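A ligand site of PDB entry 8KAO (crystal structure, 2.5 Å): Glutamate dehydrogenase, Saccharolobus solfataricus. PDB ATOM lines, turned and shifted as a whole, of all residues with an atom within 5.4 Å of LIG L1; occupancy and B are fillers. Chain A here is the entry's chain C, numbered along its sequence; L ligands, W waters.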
ATOM      1  N   GLY A  74      -9.852 -23.345  -6.976  1.00  0.00           N
ATOM      2  CA  GLY A  74     -10.757 -22.291  -6.566  1.00  0.00           C
ATOM      3  C   GLY A  74     -12.084 -22.777  -5.997  1.00  0.00           C
ATOM      4  O   GLY A  74     -12.385 -23.968  -5.999  1.00  0.00           O
ATOM      5  N   ARG A  76     -16.195 -21.611  -6.439  1.00  0.00           N
ATOM      6  CA  ARG A  76     -17.152 -20.726  -7.084  1.00  0.00           C
ATOM      7  C   ARG A  76     -18.464 -20.678  -6.293  1.00  0.00           C
ATOM      8  O   ARG A  76     -18.947 -21.684  -5.810  1.00  0.00           O
ATOM      9  CB  ARG A  76     -17.438 -21.051  -8.554  1.00  0.00           C
ATOM     10  CG  ARG A  76     -18.020 -22.413  -8.861  1.00  0.00           C
ATOM     11  CD  ARG A  76     -18.547 -22.470 -10.294  1.00  0.00           C
ATOM     12  NE  ARG A  76     -17.488 -22.280 -11.273  1.00  0.00           N
ATOM     13  CZ  ARG A  76     -17.564 -22.626 -12.563  1.00  0.00           C
ATOM     14  NH1 ARG A  76     -18.674 -23.147 -13.078  1.00  0.00           N
ATOM     15  NH2 ARG A  76     -16.498 -22.460 -13.336  1.00  0.00           N
ATOM     16  N   LEU A  89     -14.796 -29.843 -11.917  1.00  0.00           N
ATOM     17  CA  LEU A  89     -13.808 -28.777 -11.925  1.00  0.00           C
ATOM     18  C   LEU A  89     -12.548 -29.214 -11.175  1.00  0.00           C
ATOM     19  O   LEU A  89     -11.456 -28.701 -11.468  1.00  0.00           O
ATOM     20  CB  LEU A  89     -14.432 -27.541 -11.288  1.00  0.00           C
ATOM     21  CG  LEU A  89     -15.509 -26.851 -12.118  1.00  0.00           C
ATOM     22  CD1 LEU A  89     -16.297 -25.887 -11.235  1.00  0.00           C
ATOM     23  CD2 LEU A  89     -14.905 -26.113 -13.308  1.00  0.00           C
ATOM     24  N   LYS A 108     -11.531 -28.404  -5.954  1.00  0.00           N
ATOM     25  CA  LYS A 108     -12.318 -27.212  -6.198  1.00  0.00           C
ATOM     26  C   LYS A 108     -13.435 -27.206  -5.183  1.00  0.00           C
ATOM     27  O   LYS A 108     -13.768 -28.246  -4.635  1.00  0.00           O
ATOM     28  CB  LYS A 108     -12.912 -27.178  -7.623  1.00  0.00           C
ATOM     29  CG  LYS A 108     -12.227 -26.235  -8.598  1.00  0.00           C
ATOM     30  CD  LYS A 108     -13.123 -25.117  -9.064  1.00  0.00           C
ATOM     31  CE  LYS A 108     -12.432 -23.979  -9.771  1.00  0.00           C
ATOM     32  NZ  LYS A 108     -11.155 -24.373 -10.415  1.00  0.00           N
ATOM     33  N   PRO A 147      -9.656 -18.107  -5.542  1.00  0.00           N
ATOM     34  CA  PRO A 147     -10.871 -17.527  -6.116  1.00  0.00           C
ATOM     35  C   PRO A 147     -11.325 -18.295  -7.364  1.00  0.00           C
ATOM     36  O   PRO A 147     -10.514 -18.893  -8.089  1.00  0.00           O
ATOM     37  CB  PRO A 147     -10.443 -16.067  -6.474  1.00  0.00           C
ATOM     38  CG  PRO A 147      -9.177 -15.850  -5.654  1.00  0.00           C
ATOM     39  CD  PRO A 147      -8.504 -17.205  -5.686  1.00  0.00           C
ATOM     40  N   ASP A 148     -12.643 -18.259  -7.610  1.00  0.00           N
ATOM     41  CA  ASP A 148     -13.208 -18.718  -8.858  1.00  0.00           C
ATOM     42  C   ASP A 148     -14.280 -17.700  -9.259  1.00  0.00           C
ATOM     43  O   ASP A 148     -14.066 -16.484  -9.117  1.00  0.00           O
ATOM     44  CB  ASP A 148     -13.730 -20.149  -8.736  1.00  0.00           C
ATOM     45  CG  ASP A 148     -13.967 -20.810 -10.084  1.00  0.00           C
ATOM     46  OD1 ASP A 148     -12.984 -21.208 -10.726  1.00  0.00           O
ATOM     47  OD2 ASP A 148     -15.137 -20.902 -10.497  1.00  0.00           O
ATOM     48  N   ILE A 149     -15.428 -18.200  -9.763  1.00  0.00           N
ATOM     49  CA  ILE A 149     -16.526 -17.341 -10.160  1.00  0.00           C
ATOM     50  C   ILE A 149     -17.224 -16.810  -8.908  1.00  0.00           C
ATOM     51  O   ILE A 149     -17.505 -17.601  -7.994  1.00  0.00           O
ATOM     52  CB  ILE A 149     -17.483 -18.107 -11.089  1.00  0.00           C
ATOM     53  CG1 ILE A 149     -16.770 -18.566 -12.356  1.00  0.00           C
ATOM     54  CG2 ILE A 149     -18.715 -17.285 -11.473  1.00  0.00           C
ATOM     55  CD1 ILE A 149     -17.699 -18.889 -13.497  1.00  0.00           C
ATOM     56  N   ASN A 150     -17.470 -15.475  -8.890  1.00  0.00           N
ATOM     57  CA  ASN A 150     -18.085 -14.764  -7.770  1.00  0.00           C
ATOM     58  C   ASN A 150     -17.289 -14.906  -6.478  1.00  0.00           C
ATOM     59  O   ASN A 150     -17.863 -14.753  -5.407  1.00  0.00           O
ATOM     60  CB  ASN A 150     -19.525 -15.240  -7.571  1.00  0.00           C
ATOM     61  CG  ASN A 150     -20.431 -14.833  -8.724  1.00  0.00           C
ATOM     62  OD1 ASN A 150     -20.177 -13.826  -9.382  1.00  0.00           O
ATOM     63  ND2 ASN A 150     -21.460 -15.615  -8.994  1.00  0.00           N
ATOM     64  N   THR A 151     -15.993 -15.214  -6.579  1.00  0.00           N
ATOM     65  CA  THR A 151     -15.112 -15.216  -5.408  1.00  0.00           C
ATOM     66  C   THR A 151     -13.906 -14.384  -5.816  1.00  0.00           C
ATOM     67  O   THR A 151     -13.600 -14.256  -6.999  1.00  0.00           O
ATOM     68  CB  THR A 151     -14.690 -16.613  -4.913  1.00  0.00           C
ATOM     69  OG1 THR A 151     -14.328 -17.457  -6.019  1.00  0.00           O
ATOM     70  CG2 THR A 151     -15.835 -17.264  -4.156  1.00  0.00           C
ATOM     71  N   ARG A 188      -1.253 -11.889  -9.086  1.00  0.00           N
ATOM     72  CA  ARG A 188      -2.275 -12.921  -9.026  1.00  0.00           C
ATOM     73  C   ARG A 188      -3.624 -12.352  -9.461  1.00  0.00           C
ATOM     74  O   ARG A 188      -4.443 -13.076 -10.036  1.00  0.00           O
ATOM     75  CB  ARG A 188      -2.296 -13.527  -7.625  1.00  0.00           C
ATOM     76  CG  ARG A 188      -3.338 -14.621  -7.478  1.00  0.00           C
ATOM     77  CD  ARG A 188      -3.176 -15.747  -8.487  1.00  0.00           C
ATOM     78  NE  ARG A 188      -4.296 -16.672  -8.406  1.00  0.00           N
ATOM     79  CZ  ARG A 188      -5.353 -16.603  -9.199  1.00  0.00           C
ATOM     80  NH1 ARG A 188      -5.381 -15.676 -10.143  1.00  0.00           N
ATOM     81  NH2 ARG A 188      -6.372 -17.434  -9.034  1.00  0.00           N
ATOM     82  N   THR A 192      -4.363 -14.905 -14.482  1.00  0.00           N
ATOM     83  CA  THR A 192      -5.105 -15.787 -15.365  1.00  0.00           C
ATOM     84  C   THR A 192      -5.259 -15.140 -16.735  1.00  0.00           C
ATOM     85  O   THR A 192      -4.895 -15.765 -17.720  1.00  0.00           O
ATOM     86  CB  THR A 192      -6.460 -16.186 -14.804  1.00  0.00           C
ATOM     87  OG1 THR A 192      -6.263 -16.585 -13.457  1.00  0.00           O
ATOM     88  CG2 THR A 192      -7.060 -17.337 -15.576  1.00  0.00           C
ATOM     89  N   GLN A 219     -16.042 -14.285 -24.489  1.00  0.00           N
ATOM     90  CA  GLN A 219     -17.268 -14.465 -23.743  1.00  0.00           C
ATOM     91  C   GLN A 219     -16.913 -14.448 -22.270  1.00  0.00           C
ATOM     92  O   GLN A 219     -16.002 -15.165 -21.862  1.00  0.00           O
ATOM     93  CB  GLN A 219     -17.949 -15.789 -24.075  1.00  0.00           C
ATOM     94  CG  GLN A 219     -19.033 -16.164 -23.078  1.00  0.00           C
ATOM     95  CD  GLN A 219     -19.614 -17.513 -23.403  1.00  0.00           C
ATOM     96  OE1 GLN A 219     -18.865 -18.454 -23.678  1.00  0.00           O
ATOM     97  NE2 GLN A 219     -20.943 -17.617 -23.409  1.00  0.00           N
ATOM     98  N   GLY A 220     -17.597 -13.588 -21.498  1.00  0.00           N
ATOM     99  CA  GLY A 220     -17.219 -13.316 -20.115  1.00  0.00           C
ATOM    100  C   GLY A 220     -16.337 -12.077 -20.025  1.00  0.00           C
ATOM    101  O   GLY A 220     -15.458 -11.856 -20.851  1.00  0.00           O
ATOM    102  N   PHE A 221     -16.590 -11.265 -18.992  1.00  0.00           N
ATOM    103  CA  PHE A 221     -15.831 -10.045 -18.783  1.00  0.00           C
ATOM    104  C   PHE A 221     -15.510  -9.814 -17.303  1.00  0.00           C
ATOM    105  O   PHE A 221     -15.335  -8.685 -16.882  1.00  0.00           O
ATOM    106  CB  PHE A 221     -16.615  -8.853 -19.331  1.00  0.00           C
ATOM    107  CG  PHE A 221     -15.756  -7.738 -19.867  1.00  0.00           C
ATOM    108  CD1 PHE A 221     -14.849  -7.970 -20.890  1.00  0.00           C
ATOM    109  CD2 PHE A 221     -15.875  -6.452 -19.380  1.00  0.00           C
ATOM    110  CE1 PHE A 221     -14.062  -6.943 -21.410  1.00  0.00           C
ATOM    111  CE2 PHE A 221     -15.099  -5.421 -19.893  1.00  0.00           C
ATOM    112  CZ  PHE A 221     -14.195  -5.670 -20.911  1.00  0.00           C
ATOM    113  N   GLY A 222     -15.349 -10.903 -16.544  1.00  0.00           N
ATOM    114  CA  GLY A 222     -14.939 -10.818 -15.162  1.00  0.00           C
ATOM    115  C   GLY A 222     -13.417 -10.850 -15.021  1.00  0.00           C
ATOM    116  O   GLY A 222     -12.704 -10.254 -15.817  1.00  0.00           O
ATOM    117  N   ASN A 223     -12.930 -11.520 -13.981  1.00  0.00           N
ATOM    118  CA  ASN A 223     -11.510 -11.427 -13.639  1.00  0.00           C
ATOM    119  C   ASN A 223     -10.649 -12.023 -14.760  1.00  0.00           C
ATOM    120  O   ASN A 223      -9.517 -11.593 -14.943  1.00  0.00           O
ATOM    121  CB  ASN A 223     -11.201 -12.106 -12.294  1.00  0.00           C
ATOM    122  CG  ASN A 223      -9.719 -12.211 -12.011  1.00  0.00           C
ATOM    123  OD1 ASN A 223      -9.140 -13.292 -12.092  1.00  0.00           O
ATOM    124  ND2 ASN A 223      -9.073 -11.091 -11.706  1.00  0.00           N
ATOM    125  N   VAL A 224     -11.145 -13.059 -15.441  1.00  0.00           N
ATOM    126  CA  VAL A 224     -10.412 -13.681 -16.529  1.00  0.00           C
ATOM    127  C   VAL A 224     -10.594 -12.869 -17.812  1.00  0.00           C
ATOM    128  O   VAL A 224      -9.619 -12.543 -18.484  1.00  0.00           O
ATOM    129  CB  VAL A 224     -10.858 -15.137 -16.776  1.00  0.00           C
ATOM    130  CG1 VAL A 224     -10.304 -15.697 -18.075  1.00  0.00           C
ATOM    131  CG2 VAL A 224     -10.461 -16.027 -15.621  1.00  0.00           C
ATOM    132  N   GLY A 225     -11.855 -12.636 -18.186  1.00  0.00           N
ATOM    133  CA  GLY A 225     -12.193 -12.051 -19.472  1.00  0.00           C
ATOM    134  C   GLY A 225     -11.712 -10.610 -19.623  1.00  0.00           C
ATOM    135  O   GLY A 225     -11.205 -10.214 -20.684  1.00  0.00           O
ATOM    136  N   SER A 243     -18.805  -9.964 -23.739  1.00  0.00           N
ATOM    137  CA  SER A 243     -20.112 -10.318 -23.210  1.00  0.00           C
ATOM    138  C   SER A 243     -19.985 -10.711 -21.756  1.00  0.00           C
ATOM    139  O   SER A 243     -18.885 -10.941 -21.252  1.00  0.00           O
ATOM    140  CB  SER A 243     -20.741 -11.442 -23.987  1.00  0.00           C
ATOM    141  OG  SER A 243     -20.302 -12.706 -23.510  1.00  0.00           O
ATOM    142  N   ASP A 244     -21.135 -10.766 -21.081  1.00  0.00           N
ATOM    143  CA  ASP A 244     -21.223 -11.292 -19.735  1.00  0.00           C
ATOM    144  C   ASP A 244     -22.592 -11.943 -19.617  1.00  0.00           C
ATOM    145  O   ASP A 244     -23.231 -12.213 -20.640  1.00  0.00           O
ATOM    146  CB  ASP A 244     -20.874 -10.207 -18.702  1.00  0.00           C
ATOM    147  CG  ASP A 244     -21.667  -8.910 -18.763  1.00  0.00           C
ATOM    148  OD1 ASP A 244     -22.903  -8.975 -18.920  1.00  0.00           O
ATOM    149  OD2 ASP A 244     -21.049  -7.844 -18.572  1.00  0.00           O
ATOM    150  N   ILE A 245     -23.036 -12.192 -18.381  1.00  0.00           N
ATOM    151  CA  ILE A 245     -24.324 -12.807 -18.139  1.00  0.00           C
ATOM    152  C   ILE A 245     -25.410 -11.998 -18.841  1.00  0.00           C
ATOM    153  O   ILE A 245     -26.380 -12.572 -19.337  1.00  0.00           O
ATOM    154  CB  ILE A 245     -24.563 -12.972 -16.619  1.00  0.00           C
ATOM    155  CG1 ILE A 245     -25.633 -14.018 -16.307  1.00  0.00           C
ATOM    156  CG2 ILE A 245     -24.850 -11.634 -15.942  1.00  0.00           C
ATOM    157  CD1 ILE A 245     -25.323 -14.848 -15.059  1.00  0.00           C
ATOM    158  N   GLY A 246     -25.227 -10.672 -18.935  1.00  0.00           N
ATOM    159  CA  GLY A 246     -26.251  -9.782 -19.495  1.00  0.00           C
ATOM    160  C   GLY A 246     -26.371  -9.839 -21.026  1.00  0.00           C
ATOM    161  O   GLY A 246     -27.314  -9.244 -21.574  1.00  0.00           O
ATOM    162  N   ASN A 281     -25.462 -14.372 -26.063  1.00  0.00           N
ATOM    163  CA  ASN A 281     -24.233 -15.129 -25.846  1.00  0.00           C
ATOM    164  C   ASN A 281     -24.082 -16.143 -26.975  1.00  0.00           C
ATOM    165  O   ASN A 281     -23.012 -16.272 -27.553  1.00  0.00           O
ATOM    166  CB  ASN A 281     -24.176 -15.692 -24.426  1.00  0.00           C
ATOM    167  CG  ASN A 281     -23.443 -14.750 -23.493  1.00  0.00           C
ATOM    168  OD1 ASN A 281     -22.212 -14.743 -23.452  1.00  0.00           O
ATOM    169  ND2 ASN A 281     -24.178 -13.937 -22.762  1.00  0.00           N
ATOM    170  N   ALA A 295     -14.442 -17.255 -21.736  1.00  0.00           N
ATOM    171  CA  ALA A 295     -13.813 -16.887 -20.475  1.00  0.00           C
ATOM    172  C   ALA A 295     -14.880 -16.712 -19.401  1.00  0.00           C
ATOM    173  O   ALA A 295     -14.757 -15.834 -18.564  1.00  0.00           O
ATOM    174  CB  ALA A 295     -13.020 -15.617 -20.630  1.00  0.00           C
ATOM    175  N   ALA A 296     -15.909 -17.564 -19.436  1.00  0.00           N
ATOM    176  CA  ALA A 296     -17.019 -17.448 -18.497  1.00  0.00           C
ATOM    177  C   ALA A 296     -17.286 -18.808 -17.847  1.00  0.00           C
ATOM    178  O   ALA A 296     -16.754 -19.084 -16.769  1.00  0.00           O
ATOM    179  CB  ALA A 296     -18.216 -16.908 -19.215  1.00  0.00           C
ATOM    180  N   VAL A 297     -18.104 -19.640 -18.517  1.00  0.00           N
ATOM    181  CA  VAL A 297     -18.597 -20.884 -17.921  1.00  0.00           C
ATOM    182  C   VAL A 297     -18.380 -22.059 -18.883  1.00  0.00           C
ATOM    183  O   VAL A 297     -17.949 -21.879 -20.032  1.00  0.00           O
ATOM    184  CB  VAL A 297     -20.065 -20.761 -17.465  1.00  0.00           C
ATOM    185  CG1 VAL A 297     -20.229 -19.747 -16.342  1.00  0.00           C
ATOM    186  CG2 VAL A 297     -20.994 -20.423 -18.618  1.00  0.00           C
ATOM    187  N   GLU A 298     -18.667 -23.266 -18.380  1.00  0.00           N
ATOM    188  CA  GLU A 298     -18.442 -24.513 -19.093  1.00  0.00           C
ATOM    189  C   GLU A 298     -19.543 -24.859 -20.095  1.00  0.00           C
ATOM    190  O   GLU A 298     -20.658 -24.350 -20.022  1.00  0.00           O
ATOM    191  CB  GLU A 298     -18.328 -25.643 -18.068  1.00  0.00           C
ATOM    192  CG  GLU A 298     -19.603 -25.948 -17.319  1.00  0.00           C
ATOM    193  CD  GLU A 298     -19.731 -25.382 -15.908  1.00  0.00           C
ATOM    194  OE1 GLU A 298     -19.098 -24.348 -15.591  1.00  0.00           O
ATOM    195  OE2 GLU A 298     -20.470 -26.009 -15.123  1.00  0.00           O
ATOM    196  N   GLY A 317     -10.233 -19.746 -22.005  1.00  0.00           N
ATOM    197  CA  GLY A 317     -10.035 -19.080 -20.722  1.00  0.00           C
ATOM    198  C   GLY A 317     -10.765 -19.753 -19.563  1.00  0.00           C
ATOM    199  O   GLY A 317     -10.247 -19.860 -18.458  1.00  0.00           O
ATOM    200  N   ALA A 318     -12.008 -20.170 -19.818  1.00  0.00           N
ATOM    201  CA  ALA A 318     -12.854 -20.790 -18.805  1.00  0.00           C
ATOM    202  C   ALA A 318     -12.492 -22.260 -18.646  1.00  0.00           C
ATOM    203  O   ALA A 318     -11.923 -22.887 -19.550  1.00  0.00           O
ATOM    204  CB  ALA A 318     -14.292 -20.640 -19.237  1.00  0.00           C
ATOM    205  N   ASN A 319     -12.846 -22.829 -17.494  1.00  0.00           N
ATOM    206  CA  ASN A 319     -12.705 -24.271 -17.274  1.00  0.00           C
ATOM    207  C   ASN A 319     -13.826 -24.995 -18.003  1.00  0.00           C
ATOM    208  O   ASN A 319     -14.991 -24.663 -17.816  1.00  0.00           O
ATOM    209  CB  ASN A 319     -12.770 -24.611 -15.783  1.00  0.00           C
ATOM    210  CG  ASN A 319     -11.570 -24.092 -15.024  1.00  0.00           C
ATOM    211  OD1 ASN A 319     -10.472 -24.577 -15.251  1.00  0.00           O
ATOM    212  ND2 ASN A 319     -11.765 -23.118 -14.153  1.00  0.00           N
ATOM    213  N   ASN A 344      -5.679 -21.308 -19.027  1.00  0.00           N
ATOM    214  CA  ASN A 344      -6.067 -20.563 -17.839  1.00  0.00           C
ATOM    215  C   ASN A 344      -5.171 -20.885 -16.650  1.00  0.00           C
ATOM    216  O   ASN A 344      -5.475 -20.505 -15.518  1.00  0.00           O
ATOM    217  CB  ASN A 344      -7.536 -20.835 -17.505  1.00  0.00           C
ATOM    218  CG  ASN A 344      -7.715 -21.976 -16.527  1.00  0.00           C
ATOM    219  OD1 ASN A 344      -7.631 -23.142 -16.898  1.00  0.00           O
ATOM    220  ND2 ASN A 344      -7.979 -21.631 -15.270  1.00  0.00           N
ATOM    221  N   GLY A 347      -3.625 -18.631 -13.613  1.00  0.00           N
ATOM    222  CA  GLY A 347      -4.204 -18.563 -12.281  1.00  0.00           C
ATOM    223  C   GLY A 347      -3.397 -19.389 -11.295  1.00  0.00           C
ATOM    224  O   GLY A 347      -2.804 -18.848 -10.368  1.00  0.00           O
HETATM  225  P1  LIG L   1     -15.768 -13.727 -12.450  1.00  0.00           P
HETATM  226  O1  LIG L   1     -16.799 -14.035 -11.402  1.00  0.00           O
HETATM  227  O2  LIG L   1     -14.649 -12.773 -12.171  1.00  0.00           O
HETATM  228  O3  LIG L   1     -16.499 -13.228 -13.776  1.00  0.00           O
HETATM  229  C1  LIG L   1     -17.491 -14.044 -14.400  1.00  0.00           C
HETATM  230  C2  LIG L   1     -17.799 -13.387 -15.717  1.00  0.00           C
HETATM  231  O4  LIG L   1     -18.538 -14.314 -16.543  1.00  0.00           O
HETATM  232  C3  LIG L   1     -18.685 -12.140 -15.608  1.00  0.00           C
HETATM  233  O5  LIG L   1     -18.531 -11.275 -16.726  1.00  0.00           O
HETATM  234  C4  LIG L   1     -20.069 -12.773 -15.679  1.00  0.00           C
HETATM  235  O6  LIG L   1     -21.089 -11.816 -15.934  1.00  0.00           O
HETATM  236  C5  LIG L   1     -19.809 -13.759 -16.802  1.00  0.00           C
HETATM  237  N1  LIG L   1     -20.794 -14.838 -16.879  1.00  0.00           N
HETATM  238  C6  LIG L   1     -21.376 -15.493 -15.825  1.00  0.00           C
HETATM  239  N2  LIG L   1     -22.291 -16.366 -16.195  1.00  0.00           N
HETATM  240  C7  LIG L   1     -22.299 -16.276 -17.586  1.00  0.00           C
HETATM  241  C8  LIG L   1     -23.027 -16.944 -18.576  1.00  0.00           C
HETATM  242  N3  LIG L   1     -23.925 -17.889 -18.307  1.00  0.00           N
HETATM  243  N4  LIG L   1     -22.788 -16.646 -19.876  1.00  0.00           N
HETATM  244  C9  LIG L   1     -21.880 -15.690 -20.149  1.00  0.00           C
HETATM  245  N5  LIG L   1     -21.130 -14.983 -19.298  1.00  0.00           N
HETATM  246  C10 LIG L   1     -21.381 -15.328 -18.020  1.00  0.00           C
HETATM  247  O7  LIG L   1     -15.212 -15.166 -12.861  1.00  0.00           O
HETATM  248  P2  LIG L   1     -13.776 -15.529 -13.460  1.00  0.00           P
HETATM  249  O8  LIG L   1     -12.841 -15.683 -12.300  1.00  0.00           O
HETATM  250  O9  LIG L   1     -13.493 -14.539 -14.564  1.00  0.00           O
HETATM  251  O10 LIG L   1     -14.088 -16.969 -14.112  1.00  0.00           O
HETATM  252  C11 LIG L   1     -13.828 -17.131 -15.532  1.00  0.00           C
HETATM  253  C12 LIG L   1     -13.475 -18.570 -15.824  1.00  0.00           C
HETATM  254  O11 LIG L   1     -12.092 -18.836 -15.458  1.00  0.00           O
HETATM  255  C13 LIG L   1     -14.361 -19.582 -15.079  1.00  0.00           C
HETATM  256  O12 LIG L   1     -14.761 -20.663 -15.902  1.00  0.00           O
HETATM  257  C14 LIG L   1     -13.477 -20.025 -13.914  1.00  0.00           C
HETATM  258  O13 LIG L   1     -13.693 -21.376 -13.552  1.00  0.00           O
HETATM  259  C15 LIG L   1     -12.048 -19.837 -14.449  1.00  0.00           C
HETATM  260  N6  LIG L   1     -11.175 -19.453 -13.293  1.00  0.00           N
HETATM  261  C16 LIG L   1     -10.742 -18.156 -13.036  1.00  0.00           C
HETATM  262  C17 LIG L   1      -9.966 -17.907 -11.892  1.00  0.00           C
HETATM  263  C18 LIG L   1      -9.354 -16.620 -11.455  1.00  0.00           C
HETATM  264  O14 LIG L   1      -9.457 -16.266 -10.265  1.00  0.00           O
HETATM  265  N7  LIG L   1      -8.589 -15.951 -12.306  1.00  0.00           N
HETATM  266  C19 LIG L   1      -9.662 -18.937 -11.007  1.00  0.00           C
HETATM  267  C20 LIG L   1     -10.136 -20.202 -11.262  1.00  0.00           C
HETATM  268  C21 LIG L   1     -10.898 -20.447 -12.386  1.00  0.00           C
HETATM  269  C1  LG2 L   2      -5.558 -21.061  -8.001  1.00  0.00           C
HETATM  270  C2  LG2 L   2      -6.723 -21.966  -8.379  1.00  0.00           C
HETATM  271  C3  LG2 L   2      -7.218 -21.422  -9.700  1.00  0.00           C
HETATM  272  C4  LG2 L   2      -8.413 -22.263 -10.190  1.00  0.00           C
HETATM  273  O1  LG2 L   2      -9.213 -22.873  -9.442  1.00  0.00           O
HETATM  274  C5  LG2 L   2      -8.566 -22.426 -11.703  1.00  0.00           C
HETATM  275  O2  LG2 L   2      -7.680 -21.911 -12.497  1.00  0.00           O
HETATM  276  O3  LG2 L   2      -9.545 -23.144 -12.135  1.00  0.00           O
HETATM  277  O   HOH W   1      -6.458 -13.772 -11.958  1.00  0.00           O
HETATM  278  O   HOH W   2     -21.826 -10.449 -14.070  1.00  0.00           O
HETATM  279  O   HOH W   3     -16.236 -23.200 -16.154  1.00  0.00           O
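The backbone NH (N) of Asn 319 lies within hydrogen-bond range of an oxygen (O12) of LIG L1 (3.3 Å). An oxygen (O13) of LIG L1 is in hydrogen-bond range of the side-chain amide nitrogen (ND2) of Asn 319. The side-chain hydroxyl (OG1) of Thr 192 sits at hydrogen-bond distance from a nitrogen (N7) of LIG L1, 2.7 Å away. The backbone carbonyl oxygen (O) of Ala 296 is in hydrogen-bond range of an oxygen (O12) of LIG L1 (2.7 Å). N of Asn 223 sits at hydrogen-bond distance from O2 of LIG L1 (2.8 Å). The side-chain amide oxygen (OD1) of Asn 223 sits at hydrogen-bond distance from a nitrogen (N7) of LIG L1 (2.7 Å). An oxygen (O13) of LIG L1 sits close to the side-chain carboxylate (OD1) of Asp 148, 2.9 Å away. The backbone NH of Val 224 sits at hydrogen-bond distance from an oxygen (O9) of LIG L1. The backbone NH of Asn 150 lies within hydrogen-bond range of an oxygen (O1) of LIG L1, at 3.0 Å. N of Phe 221 sits at hydrogen-bond distance from O5 of LIG L1 (3.0 Å). An oxygen (O13) of LIG L1 is in hydrogen-bond range of the guanidinium group (NH2) of Arg 76 (3.0 Å). An oxygen (O6) of LIG L1 is in hydrogen-bond range of the backbone NH (N) of Ile 245. N of Gly 222 lies within hydrogen-bond range of O5 of LIG L1, 3.2 Å away. The side-chain amide nitrogen of Asn 319 is in hydrogen-bond range of an oxygen (O3) of LG2 L2, 3.0 Å away. The side-chain amide nitrogen (ND2) of Asn 344 sits at hydrogen-bond distance from an oxygen (O2) of LG2 L2. The side-chain amino group (NZ) of Lys 108 is in salt-bridge range of an oxygen (O3) of LG2 L2, at 2.7 Å. N of Gly 74 is in hydrogen-bond range of O1 of LG2 L2 (2.6 Å).
OG1 of Thr 192 lies close to N of Gly 347. The backbone carbonyl oxygen (O) of Gln 219 sits at hydrogen-bond distance from the backbone NH (N) of Ala 296 (3.4 Å). NE of Arg 76 is in salt-bridge range of OD2 of Asp 148 (2.8 Å). The side-chain amino group (NZ) of Lys 108 is in salt-bridge range of the side-chain carboxylate (OD1) of Asp 148 (3.7 Å). NH1 of Arg 76 is in salt-bridge range of OE1 of Glu 298 (2.8 Å). The side-chain carboxylate (OD1) of Asp 244 is in hydrogen-bond range of the backbone NH (N) of Gly 246, at 2.9 Å. The side-chain amide oxygen (OD1) of Asn 281 sits at hydrogen-bond distance from the side-chain amide nitrogen (NE2) of Gln 219 (3.1 Å). O of Ser 243 sits at hydrogen-bond distance from N of Gly 220, 3.0 Å away.
Residues that only touch LIG L1: Pro 147, Asp 244, Ala 318, Ala 295, Asn 281, Arg 188, Ile 149, Gly 317, Val 297, Gln 219 and Gly 220. Of the 32 residues printed, 22 come within 4 Å of LIG L1. The nearest printed residue that does not touch LIG L1 is Asn 344 (4.3 Å).
Water W3 lies within hydrogen-bond range of the backbone carbonyl oxygen of Asn 319, the guanidinium group of Arg 76, an oxygen (O12) of LIG L1 and the side-chain carboxylate of Glu 298. Water W1 lies within hydrogen-bond range of OD1 of Asn 223 (2.7 Å), NH1 of Arg 188 (2.8 Å), N7 of LIG L1 (3.1 Å) and OG1 of Thr 192 (3.2 Å).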
